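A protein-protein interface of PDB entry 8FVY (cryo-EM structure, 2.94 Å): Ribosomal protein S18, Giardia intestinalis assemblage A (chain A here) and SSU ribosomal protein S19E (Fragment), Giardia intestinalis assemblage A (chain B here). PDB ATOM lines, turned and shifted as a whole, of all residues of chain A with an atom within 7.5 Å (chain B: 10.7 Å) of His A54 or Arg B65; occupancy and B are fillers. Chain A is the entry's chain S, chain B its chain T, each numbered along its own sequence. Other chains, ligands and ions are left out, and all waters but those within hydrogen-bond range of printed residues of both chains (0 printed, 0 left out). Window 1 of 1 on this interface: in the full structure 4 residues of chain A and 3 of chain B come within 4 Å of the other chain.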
ATOM      1  N   MET A   1       6.363   7.032   6.000  1.00  0.00           N
ATOM      2  CA  MET A   1       4.997   6.493   6.221  1.00  0.00           C
ATOM      3  C   MET A   1       5.138   5.147   6.900  1.00  0.00           C
ATOM      4  O   MET A   1       6.251   4.682   7.139  1.00  0.00           O
ATOM      5  CB  MET A   1       4.238   6.357   4.907  1.00  0.00           C
ATOM      6  CG  MET A   1       3.749   7.674   4.356  1.00  0.00           C
ATOM      7  SD  MET A   1       2.058   7.711   3.754  1.00  0.00           S
ATOM      8  CE  MET A   1       2.159   9.146   2.687  1.00  0.00           C
ATOM      9  N   THR A   2       4.013   4.515   7.206  1.00  0.00           N
ATOM     10  CA  THR A   2       4.028   3.288   7.986  1.00  0.00           C
ATOM     11  C   THR A   2       4.674   3.538   9.343  1.00  0.00           C
ATOM     12  O   THR A   2       5.305   2.659   9.931  1.00  0.00           O
ATOM     13  CB  THR A   2       4.751   2.170   7.243  1.00  0.00           C
ATOM     14  OG1 THR A   2       4.470   2.267   5.843  1.00  0.00           O
ATOM     15  CG2 THR A   2       4.306   0.801   7.754  1.00  0.00           C
ATOM     16  N   THR A   3       4.526   4.761   9.834  1.00  0.00           N
ATOM     17  CA  THR A   3       4.950   5.143  11.174  1.00  0.00           C
ATOM     18  C   THR A   3       3.672   5.378  11.954  1.00  0.00           C
ATOM     19  O   THR A   3       3.071   6.449  11.880  1.00  0.00           O
ATOM     20  CB  THR A   3       5.840   6.363  11.178  1.00  0.00           C
ATOM     21  OG1 THR A   3       5.047   7.546  11.067  1.00  0.00           O
ATOM     22  CG2 THR A   3       6.834   6.321  10.059  1.00  0.00           C
ATOM     23  N   VAL A  26       3.133  17.318   9.174  1.00  0.00           N
ATOM     24  CA  VAL A  26       4.155  16.831   8.274  1.00  0.00           C
ATOM     25  C   VAL A  26       5.264  17.856   8.202  1.00  0.00           C
ATOM     26  O   VAL A  26       5.061  19.053   8.423  1.00  0.00           O
ATOM     27  CB  VAL A  26       3.595  16.522   6.879  1.00  0.00           C
ATOM     28  CG1 VAL A  26       2.474  15.555   6.983  1.00  0.00           C
ATOM     29  CG2 VAL A  26       3.153  17.758   6.226  1.00  0.00           C
ATOM     30  N   LEU A  27       6.454  17.371   7.893  1.00  0.00           N
ATOM     31  CA  LEU A  27       7.659  18.139   8.138  1.00  0.00           C
ATOM     32  C   LEU A  27       7.686  19.417   7.315  1.00  0.00           C
ATOM     33  O   LEU A  27       7.891  20.511   7.848  1.00  0.00           O
ATOM     34  CB  LEU A  27       8.851  17.260   7.832  1.00  0.00           C
ATOM     35  CG  LEU A  27      10.242  17.724   8.151  1.00  0.00           C
ATOM     36  CD1 LEU A  27      10.285  18.521   9.365  1.00  0.00           C
ATOM     37  CD2 LEU A  27      11.032  16.526   8.333  1.00  0.00           C
ATOM     38  N   GLU A  28       7.456  19.300   6.016  1.00  0.00           N
ATOM     39  CA  GLU A  28       7.649  20.425   5.119  1.00  0.00           C
ATOM     40  C   GLU A  28       6.615  21.523   5.292  1.00  0.00           C
ATOM     41  O   GLU A  28       6.811  22.622   4.769  1.00  0.00           O
ATOM     42  CB  GLU A  28       7.662  19.933   3.680  1.00  0.00           C
ATOM     43  CG  GLU A  28       6.444  19.150   3.246  1.00  0.00           C
ATOM     44  CD  GLU A  28       5.216  19.995   3.078  1.00  0.00           C
ATOM     45  OE1 GLU A  28       5.356  21.168   2.682  1.00  0.00           O
ATOM     46  OE2 GLU A  28       4.108  19.476   3.321  1.00  0.00           O
ATOM     47  N   ARG A  39       7.038  26.705   1.235  1.00  0.00           N
ATOM     48  CA  ARG A  39       6.906  25.345   0.730  1.00  0.00           C
ATOM     49  C   ARG A  39       7.998  25.017  -0.268  1.00  0.00           C
ATOM     50  O   ARG A  39       8.599  23.941  -0.214  1.00  0.00           O
ATOM     51  CB  ARG A  39       5.545  25.159   0.081  1.00  0.00           C
ATOM     52  CG  ARG A  39       4.432  24.981   1.055  1.00  0.00           C
ATOM     53  CD  ARG A  39       4.444  23.623   1.659  1.00  0.00           C
ATOM     54  NE  ARG A  39       4.045  22.599   0.710  1.00  0.00           N
ATOM     55  CZ  ARG A  39       2.783  22.302   0.444  1.00  0.00           C
ATOM     56  NH1 ARG A  39       1.789  22.971   0.993  1.00  0.00           N
ATOM     57  NH2 ARG A  39       2.513  21.308  -0.390  1.00  0.00           N
ATOM     58  N   LEU A  46      15.416  20.162   2.332  1.00  0.00           N
ATOM     59  CA  LEU A  46      15.423  18.840   2.934  1.00  0.00           C
ATOM     60  C   LEU A  46      16.009  17.822   1.981  1.00  0.00           C
ATOM     61  O   LEU A  46      16.903  17.048   2.338  1.00  0.00           O
ATOM     62  CB  LEU A  46      14.014  18.424   3.307  1.00  0.00           C
ATOM     63  CG  LEU A  46      13.058  19.398   3.970  1.00  0.00           C
ATOM     64  CD1 LEU A  46      11.640  19.031   3.655  1.00  0.00           C
ATOM     65  CD2 LEU A  46      13.214  19.389   5.418  1.00  0.00           C
ATOM     66  N   LYS A  47      15.520  17.825   0.748  1.00  0.00           N
ATOM     67  CA  LYS A  47      15.911  16.813  -0.215  1.00  0.00           C
ATOM     68  C   LYS A  47      17.420  16.748  -0.338  1.00  0.00           C
ATOM     69  O   LYS A  47      18.014  15.667  -0.317  1.00  0.00           O
ATOM     70  CB  LYS A  47      15.278  17.131  -1.556  1.00  0.00           C
ATOM     71  CG  LYS A  47      14.426  16.035  -2.090  1.00  0.00           C
ATOM     72  CD  LYS A  47      13.731  16.440  -3.374  1.00  0.00           C
ATOM     73  CE  LYS A  47      12.671  17.473  -3.153  1.00  0.00           C
ATOM     74  NZ  LYS A  47      12.049  17.880  -4.436  1.00  0.00           N
ATOM     75  N   ILE A  51      16.656  13.787   3.702  1.00  0.00           N
ATOM     76  CA  ILE A  51      15.611  13.698   4.707  1.00  0.00           C
ATOM     77  C   ILE A  51      14.310  13.364   4.005  1.00  0.00           C
ATOM     78  O   ILE A  51      14.032  13.880   2.919  1.00  0.00           O
ATOM     79  CB  ILE A  51      15.465  15.008   5.498  1.00  0.00           C
ATOM     80  CG1 ILE A  51      16.726  15.335   6.272  1.00  0.00           C
ATOM     81  CG2 ILE A  51      14.361  14.899   6.449  1.00  0.00           C
ATOM     82  CD1 ILE A  51      16.756  16.745   6.783  1.00  0.00           C
ATOM     83  N   ASP A  52      13.519  12.496   4.619  1.00  0.00           N
ATOM     84  CA  ASP A  52      12.200  12.216   4.088  1.00  0.00           C
ATOM     85  C   ASP A  52      11.294  13.415   4.284  1.00  0.00           C
ATOM     86  O   ASP A  52      11.430  14.178   5.242  1.00  0.00           O
ATOM     87  CB  ASP A  52      11.595  10.994   4.748  1.00  0.00           C
ATOM     88  CG  ASP A  52      10.284  10.607   4.129  1.00  0.00           C
ATOM     89  OD1 ASP A  52       9.921  11.223   3.107  1.00  0.00           O
ATOM     90  OD2 ASP A  52       9.619   9.690   4.654  1.00  0.00           O
ATOM     91  N   VAL A  53      10.359  13.571   3.361  1.00  0.00           N
ATOM     92  CA  VAL A  53       9.531  14.763   3.313  1.00  0.00           C
ATOM     93  C   VAL A  53       8.103  14.483   3.742  1.00  0.00           C
ATOM     94  O   VAL A  53       7.384  15.410   4.137  1.00  0.00           O
ATOM     95  CB  VAL A  53       9.581  15.335   1.891  1.00  0.00           C
ATOM     96  CG1 VAL A  53       9.415  14.235   0.904  1.00  0.00           C
ATOM     97  CG2 VAL A  53       8.524  16.344   1.708  1.00  0.00           C
ATOM     98  N   HIS A  54       7.682  13.233   3.682  1.00  0.00           N
ATOM     99  CA  HIS A  54       6.342  12.823   4.048  1.00  0.00           C
ATOM    100  C   HIS A  54       6.409  12.154   5.404  1.00  0.00           C
ATOM    101  O   HIS A  54       5.972  11.014   5.584  1.00  0.00           O
ATOM    102  CB  HIS A  54       5.789  11.902   2.973  1.00  0.00           C
ATOM    103  CG  HIS A  54       5.520  12.601   1.681  1.00  0.00           C
ATOM    104  ND1 HIS A  54       6.019  13.853   1.397  1.00  0.00           N
ATOM    105  CD2 HIS A  54       4.831  12.213   0.583  1.00  0.00           C
ATOM    106  CE1 HIS A  54       5.625  14.217   0.191  1.00  0.00           C
ATOM    107  NE2 HIS A  54       4.908  13.238  -0.326  1.00  0.00           N
ATOM    108  N   LYS A  55       6.983  12.872   6.353  1.00  0.00           N
ATOM    109  CA  LYS A  55       7.245  12.375   7.686  1.00  0.00           C
ATOM    110  C   LYS A  55       6.757  13.377   8.704  1.00  0.00           C
ATOM    111  O   LYS A  55       6.769  14.585   8.461  1.00  0.00           O
ATOM    112  CB  LYS A  55       8.712  12.125   7.887  1.00  0.00           C
ATOM    113  CG  LYS A  55       9.021  11.475   9.175  1.00  0.00           C
ATOM    114  CD  LYS A  55      10.420  10.908   9.213  1.00  0.00           C
ATOM    115  CE  LYS A  55      11.428  11.924   9.580  1.00  0.00           C
ATOM    116  NZ  LYS A  55      11.434  12.966   8.605  1.00  0.00           N
ATOM    117  N   ARG A  56       6.314  12.863   9.834  1.00  0.00           N
ATOM    118  CA  ARG A  56       5.858  13.725  10.901  1.00  0.00           C
ATOM    119  C   ARG A  56       7.058  14.280  11.632  1.00  0.00           C
ATOM    120  O   ARG A  56       8.002  13.560  11.955  1.00  0.00           O
ATOM    121  CB  ARG A  56       4.945  12.964  11.844  1.00  0.00           C
ATOM    122  CG  ARG A  56       3.734  12.402  11.186  1.00  0.00           C
ATOM    123  CD  ARG A  56       2.785  13.469  10.760  1.00  0.00           C
ATOM    124  NE  ARG A  56       1.704  12.922   9.956  1.00  0.00           N
ATOM    125  CZ  ARG A  56       0.585  13.569   9.673  1.00  0.00           C
ATOM    126  NH1 ARG A  56       0.328  14.755  10.173  1.00  0.00           N
ATOM    127  NH2 ARG A  56      -0.311  12.999   8.886  1.00  0.00           N
ATOM    128  N   ALA A  57       7.014  15.571  11.898  1.00  0.00           N
ATOM    129  CA  ALA A  57       8.195  16.283  12.322  1.00  0.00           C
ATOM    130  C   ALA A  57       8.705  15.816  13.668  1.00  0.00           C
ATOM    131  O   ALA A  57       9.819  16.183  14.051  1.00  0.00           O
ATOM    132  CB  ALA A  57       7.881  17.755  12.347  1.00  0.00           C
ATOM    133  N   GLU A  59       9.449  12.729  14.469  1.00  0.00           N
ATOM    134  CA  GLU A  59      10.414  11.659  14.279  1.00  0.00           C
ATOM    135  C   GLU A  59      11.705  12.166  13.671  1.00  0.00           C
ATOM    136  O   GLU A  59      12.496  11.379  13.148  1.00  0.00           O
ATOM    137  CB  GLU A  59       9.841  10.542  13.414  1.00  0.00           C
ATOM    138  CG  GLU A  59       8.370  10.604  13.089  1.00  0.00           C
ATOM    139  CD  GLU A  59       8.004   9.699  11.943  1.00  0.00           C
ATOM    140  OE1 GLU A  59       8.865   8.903  11.524  1.00  0.00           O
ATOM    141  OE2 GLU A  59       6.863   9.788  11.454  1.00  0.00           O
ATOM    142  N   THR B  51      15.471  18.340 -12.602  1.00  0.00           N
ATOM    143  CA  THR B  51      14.207  17.850 -12.095  1.00  0.00           C
ATOM    144  C   THR B  51      14.045  18.064 -10.604  1.00  0.00           C
ATOM    145  O   THR B  51      12.921  17.981 -10.100  1.00  0.00           O
ATOM    146  CB  THR B  51      14.073  16.368 -12.392  1.00  0.00           C
ATOM    147  OG1 THR B  51      15.222  15.668 -11.903  1.00  0.00           O
ATOM    148  CG2 THR B  51      13.974  16.171 -13.836  1.00  0.00           C
ATOM    149  N   ASP B  52      15.126  18.340  -9.890  1.00  0.00           N
ATOM    150  CA  ASP B  52      15.056  18.359  -8.441  1.00  0.00           C
ATOM    151  C   ASP B  52      14.382  19.606  -7.903  1.00  0.00           C
ATOM    152  O   ASP B  52      14.215  19.722  -6.687  1.00  0.00           O
ATOM    153  CB  ASP B  52      16.450  18.238  -7.850  1.00  0.00           C
ATOM    154  CG  ASP B  52      16.460  17.482  -6.544  1.00  0.00           C
ATOM    155  OD1 ASP B  52      15.426  16.878  -6.198  1.00  0.00           O
ATOM    156  OD2 ASP B  52      17.502  17.492  -5.858  1.00  0.00           O
ATOM    157  N   VAL B  54      11.649  21.870  -9.938  1.00  0.00           N
ATOM    158  CA  VAL B  54      10.880  22.503 -10.998  1.00  0.00           C
ATOM    159  C   VAL B  54       9.438  22.059 -10.898  1.00  0.00           C
ATOM    160  O   VAL B  54       9.134  20.968 -10.411  1.00  0.00           O
ATOM    161  CB  VAL B  54      11.416  22.175 -12.401  1.00  0.00           C
ATOM    162  CG1 VAL B  54      12.858  22.450 -12.492  1.00  0.00           C
ATOM    163  CG2 VAL B  54      11.111  20.784 -12.745  1.00  0.00           C
ATOM    164  N   LYS B  55       8.558  22.923 -11.368  1.00  0.00           N
ATOM    165  CA  LYS B  55       7.178  22.589 -11.623  1.00  0.00           C
ATOM    166  C   LYS B  55       7.051  22.021 -13.031  1.00  0.00           C
ATOM    167  O   LYS B  55       8.038  21.836 -13.744  1.00  0.00           O
ATOM    168  CB  LYS B  55       6.319  23.825 -11.439  1.00  0.00           C
ATOM    169  CG  LYS B  55       6.575  24.508 -10.165  1.00  0.00           C
ATOM    170  CD  LYS B  55       5.641  25.649  -9.930  1.00  0.00           C
ATOM    171  CE  LYS B  55       5.850  26.775 -10.868  1.00  0.00           C
ATOM    172  NZ  LYS B  55       4.981  27.914 -10.550  1.00  0.00           N
ATOM    173  N   THR B  56       5.823  21.727 -13.441  1.00  0.00           N
ATOM    174  CA  THR B  56       5.534  21.328 -14.809  1.00  0.00           C
ATOM    175  C   THR B  56       4.670  22.347 -15.524  1.00  0.00           C
ATOM    176  O   THR B  56       4.079  22.037 -16.559  1.00  0.00           O
ATOM    177  CB  THR B  56       4.859  19.967 -14.849  1.00  0.00           C
ATOM    178  OG1 THR B  56       3.479  20.094 -14.505  1.00  0.00           O
ATOM    179  CG2 THR B  56       5.502  19.056 -13.903  1.00  0.00           C
ATOM    180  N   ARG B  60       0.719  25.561 -12.461  1.00  0.00           N
ATOM    181  CA  ARG B  60       0.846  24.809 -11.233  1.00  0.00           C
ATOM    182  C   ARG B  60       1.131  25.762 -10.080  1.00  0.00           C
ATOM    183  O   ARG B  60       0.951  26.976 -10.180  1.00  0.00           O
ATOM    184  CB  ARG B  60       1.930  23.761 -11.401  1.00  0.00           C
ATOM    185  CG  ARG B  60       1.433  22.393 -11.624  1.00  0.00           C
ATOM    186  CD  ARG B  60       0.498  22.368 -12.769  1.00  0.00           C
ATOM    187  NE  ARG B  60       0.559  21.147 -13.552  1.00  0.00           N
ATOM    188  CZ  ARG B  60       0.297  21.087 -14.848  1.00  0.00           C
ATOM    189  NH1 ARG B  60      -0.117  22.139 -15.517  1.00  0.00           N
ATOM    190  NH2 ARG B  60       0.437  19.937 -15.486  1.00  0.00           N
ATOM    191  N   GLN B  61       1.585  25.211  -8.965  1.00  0.00           N
ATOM    192  CA  GLN B  61       1.725  26.011  -7.765  1.00  0.00           C
ATOM    193  C   GLN B  61       2.776  25.427  -6.837  1.00  0.00           C
ATOM    194  O   GLN B  61       3.494  26.166  -6.164  1.00  0.00           O
ATOM    195  CB  GLN B  61       0.360  26.110  -7.110  1.00  0.00           C
ATOM    196  CG  GLN B  61       0.285  26.873  -5.845  1.00  0.00           C
ATOM    197  CD  GLN B  61      -1.121  26.919  -5.319  1.00  0.00           C
ATOM    198  OE1 GLN B  61      -1.977  26.140  -5.730  1.00  0.00           O
ATOM    199  NE2 GLN B  61      -1.373  27.830  -4.400  1.00  0.00           N
ATOM    200  N   TYR B  62       2.884  24.109  -6.811  1.00  0.00           N
ATOM    201  CA  TYR B  62       3.920  23.404  -6.084  1.00  0.00           C
ATOM    202  C   TYR B  62       4.481  22.286  -6.943  1.00  0.00           C
ATOM    203  O   TYR B  62       3.976  21.982  -8.022  1.00  0.00           O
ATOM    204  CB  TYR B  62       3.405  22.821  -4.776  1.00  0.00           C
ATOM    205  CG  TYR B  62       2.826  23.830  -3.840  1.00  0.00           C
ATOM    206  CD1 TYR B  62       3.617  24.802  -3.273  1.00  0.00           C
ATOM    207  CD2 TYR B  62       1.491  23.806  -3.516  1.00  0.00           C
ATOM    208  CE1 TYR B  62       3.097  25.720  -2.425  1.00  0.00           C
ATOM    209  CE2 TYR B  62       0.961  24.722  -2.670  1.00  0.00           C
ATOM    210  CZ  TYR B  62       1.766  25.679  -2.122  1.00  0.00           C
ATOM    211  OH  TYR B  62       1.226  26.600  -1.265  1.00  0.00           O
ATOM    212  N   ALA B  63       5.542  21.679  -6.445  1.00  0.00           N
ATOM    213  CA  ALA B  63       6.234  20.667  -7.205  1.00  0.00           C
ATOM    214  C   ALA B  63       5.630  19.288  -6.977  1.00  0.00           C
ATOM    215  O   ALA B  63       4.929  19.060  -5.992  1.00  0.00           O
ATOM    216  CB  ALA B  63       7.700  20.646  -6.834  1.00  0.00           C
ATOM    217  N   PRO B  64       5.900  18.346  -7.874  1.00  0.00           N
ATOM    218  CA  PRO B  64       5.312  17.019  -7.750  1.00  0.00           C
ATOM    219  C   PRO B  64       5.774  16.283  -6.509  1.00  0.00           C
ATOM    220  O   PRO B  64       6.902  16.442  -6.041  1.00  0.00           O
ATOM    221  CB  PRO B  64       5.785  16.320  -9.016  1.00  0.00           C
ATOM    222  CG  PRO B  64       6.095  17.380  -9.922  1.00  0.00           C
ATOM    223  CD  PRO B  64       6.622  18.470  -9.141  1.00  0.00           C
ATOM    224  N   ARG B  65       4.881  15.449  -5.997  1.00  0.00           N
ATOM    225  CA  ARG B  65       5.093  14.755  -4.744  1.00  0.00           C
ATOM    226  C   ARG B  65       5.808  13.431  -4.913  1.00  0.00           C
ATOM    227  O   ARG B  65       6.461  12.975  -3.972  1.00  0.00           O
ATOM    228  CB  ARG B  65       3.754  14.523  -4.057  1.00  0.00           C
ATOM    229  CG  ARG B  65       2.914  15.770  -3.904  1.00  0.00           C
ATOM    230  CD  ARG B  65       1.528  15.455  -3.382  1.00  0.00           C
ATOM    231  NE  ARG B  65       1.566  14.415  -2.368  1.00  0.00           N
ATOM    232  CZ  ARG B  65       2.082  14.583  -1.162  1.00  0.00           C
ATOM    233  NH1 ARG B  65       2.589  15.744  -0.786  1.00  0.00           N
ATOM    234  NH2 ARG B  65       2.091  13.563  -0.315  1.00  0.00           N
ATOM    235  N   ASP B  66       5.702  12.809  -6.076  1.00  0.00           N
ATOM    236  CA  ASP B  66       6.393  11.568  -6.362  1.00  0.00           C
ATOM    237  C   ASP B  66       7.773  11.863  -6.930  1.00  0.00           C
ATOM    238  O   ASP B  66       8.015  12.921  -7.514  1.00  0.00           O
ATOM    239  CB  ASP B  66       5.596  10.726  -7.352  1.00  0.00           C
ATOM    240  CG  ASP B  66       4.968   9.509  -6.713  1.00  0.00           C
ATOM    241  OD1 ASP B  66       4.815   9.495  -5.475  1.00  0.00           O
ATOM    242  OD2 ASP B  66       4.624   8.562  -7.451  1.00  0.00           O
ATOM    243  N   ALA B  67       8.682  10.919  -6.743  1.00  0.00           N
ATOM    244  CA  ALA B  67      10.037  11.040  -7.254  1.00  0.00           C
ATOM    245  C   ALA B  67      10.208  10.433  -8.631  1.00  0.00           C
ATOM    246  O   ALA B  67      11.298  10.526  -9.203  1.00  0.00           O
ATOM    247  CB  ALA B  67      11.014  10.371  -6.300  1.00  0.00           C
ATOM    248  N   ASP B  68       9.169   9.820  -9.177  1.00  0.00           N
ATOM    249  CA  ASP B  68       9.242   9.135 -10.450  1.00  0.00           C
ATOM    250  C   ASP B  68       8.155   9.630 -11.375  1.00  0.00           C
ATOM    251  O   ASP B  68       7.438   8.851 -12.002  1.00  0.00           O
ATOM    252  CB  ASP B  68       9.148   7.634 -10.243  1.00  0.00           C
ATOM    253  CG  ASP B  68       8.318   7.273  -9.039  1.00  0.00           C
ATOM    254  OD1 ASP B  68       7.579   8.150  -8.549  1.00  0.00           O
ATOM    255  OD2 ASP B  68       8.407   6.116  -8.579  1.00  0.00           O
ATOM    256  N   TRP B  69       8.017  10.948 -11.464  1.00  0.00           N
ATOM    257  CA  TRP B  69       7.019  11.535 -12.340  1.00  0.00           C
ATOM    258  C   TRP B  69       7.524  11.639 -13.768  1.00  0.00           C
ATOM    259  O   TRP B  69       6.728  11.655 -14.721  1.00  0.00           O
ATOM    260  CB  TRP B  69       6.617  12.899 -11.811  1.00  0.00           C
ATOM    261  CG  TRP B  69       7.734  13.837 -11.560  1.00  0.00           C
ATOM    262  CD1 TRP B  69       8.514  13.885 -10.461  1.00  0.00           C
ATOM    263  CD2 TRP B  69       8.192  14.882 -12.420  1.00  0.00           C
ATOM    264  NE1 TRP B  69       9.437  14.882 -10.576  1.00  0.00           N
ATOM    265  CE2 TRP B  69       9.257  15.510 -11.773  1.00  0.00           C
ATOM    266  CE3 TRP B  69       7.807  15.345 -13.674  1.00  0.00           C
ATOM    267  CZ2 TRP B  69       9.935  16.563 -12.327  1.00  0.00           C
ATOM    268  CZ3 TRP B  69       8.483  16.392 -14.214  1.00  0.00           C
ATOM    269  CH2 TRP B  69       9.532  16.992 -13.548  1.00  0.00           C
ATOM    270  N   PHE B  70       8.840  11.690 -13.933  1.00  0.00           N
ATOM    271  CA  PHE B  70       9.415  11.811 -15.256  1.00  0.00           C
ATOM    272  C   PHE B  70       9.035  10.635 -16.133  1.00  0.00           C
ATOM    273  O   PHE B  70       8.662  10.806 -17.298  1.00  0.00           O
ATOM    274  CB  PHE B  70      10.919  11.907 -15.132  1.00  0.00           C
ATOM    275  CG  PHE B  70      11.573  12.505 -16.315  1.00  0.00           C
ATOM    276  CD1 PHE B  70      11.594  13.865 -16.488  1.00  0.00           C
ATOM    277  CD2 PHE B  70      12.169  11.711 -17.257  1.00  0.00           C
ATOM    278  CE1 PHE B  70      12.178  14.410 -17.573  1.00  0.00           C
ATOM    279  CE2 PHE B  70      12.756  12.260 -18.343  1.00  0.00           C
ATOM    280  CZ  PHE B  70      12.763  13.609 -18.501  1.00  0.00           C
ATOM    281  N   ILE B  72       6.534   8.549 -15.784  1.00  0.00           N
ATOM    282  CA  ILE B  72       5.110   8.621 -16.071  1.00  0.00           C
ATOM    283  C   ILE B  72       4.859   9.508 -17.275  1.00  0.00           C
ATOM    284  O   ILE B  72       4.114   9.147 -18.198  1.00  0.00           O
ATOM    285  CB  ILE B  72       4.360   9.136 -14.839  1.00  0.00           C
ATOM    286  CG1 ILE B  72       4.755   8.354 -13.610  1.00  0.00           C
ATOM    287  CG2 ILE B  72       2.939   8.979 -15.022  1.00  0.00           C
ATOM    288  CD1 ILE B  72       4.700   6.915 -13.787  1.00  0.00           C
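Of the 17 printed residues of chain B, 3 touch a printed residue of chain A. Hydrophobic or aromatic side chains of chain B within 4 Å of the printed part of chain A: Tyr B62. Printed residues of chain A that touch a printed residue of chain B: Arg A39, Lys A47 and His A54. Hydrophobic or aromatic side chains of chain A within 4 Å of the printed part of chain B: His A54. Among the printed residues, Asp or Glu carboxylates within 4 Å of a Lys or Arg side-chain nitrogen of the other chain: Lys A47 with Asp B52 (3.9 Å).
A ring nitrogen (NE2) of His A54 lies within hydrogen-bond range of the guanidinium group (NH2) of Arg B65, 2.8 Å away. The side-chain amino group of Lys A47 lies within salt-bridge range of the side-chain carboxylate of Asp B52 (3.9 Å).
No residue of chain B comes within 4 Å of Met A1. Thr A2 touches none of the printed residues of chain B. No residue of chain B comes within 4 Å of Asp A52. No residue of chain B comes within 4 Å of Val A53. His A54 touches just one residue of chain B: Arg B65. No residue of chain B comes within 4 Å of Lys A55. Of the printed residues of chain A, Asp B52 touches Lys A47. Of the printed residues of chain A, Tyr B62 touches Arg A39. Of chain A, only His A54 (2.8 Å) comes within 4 Å of Arg B65. The nearest residue of chain B that does not touch His A54 is Asp B66 (5.8 Å). The nearest printed residue of chain B that does not touch Lys A47 is Pro B64 (5.6 Å).
N of His A54 is in hydrogen-bond range of OD1 of Asp A52, 3.1 Å away. The side-chain carboxylate of Glu A28 is in salt-bridge range of the guanidinium group of Arg A39 (2.8 Å).
Tyr B62 touches Arg A39.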
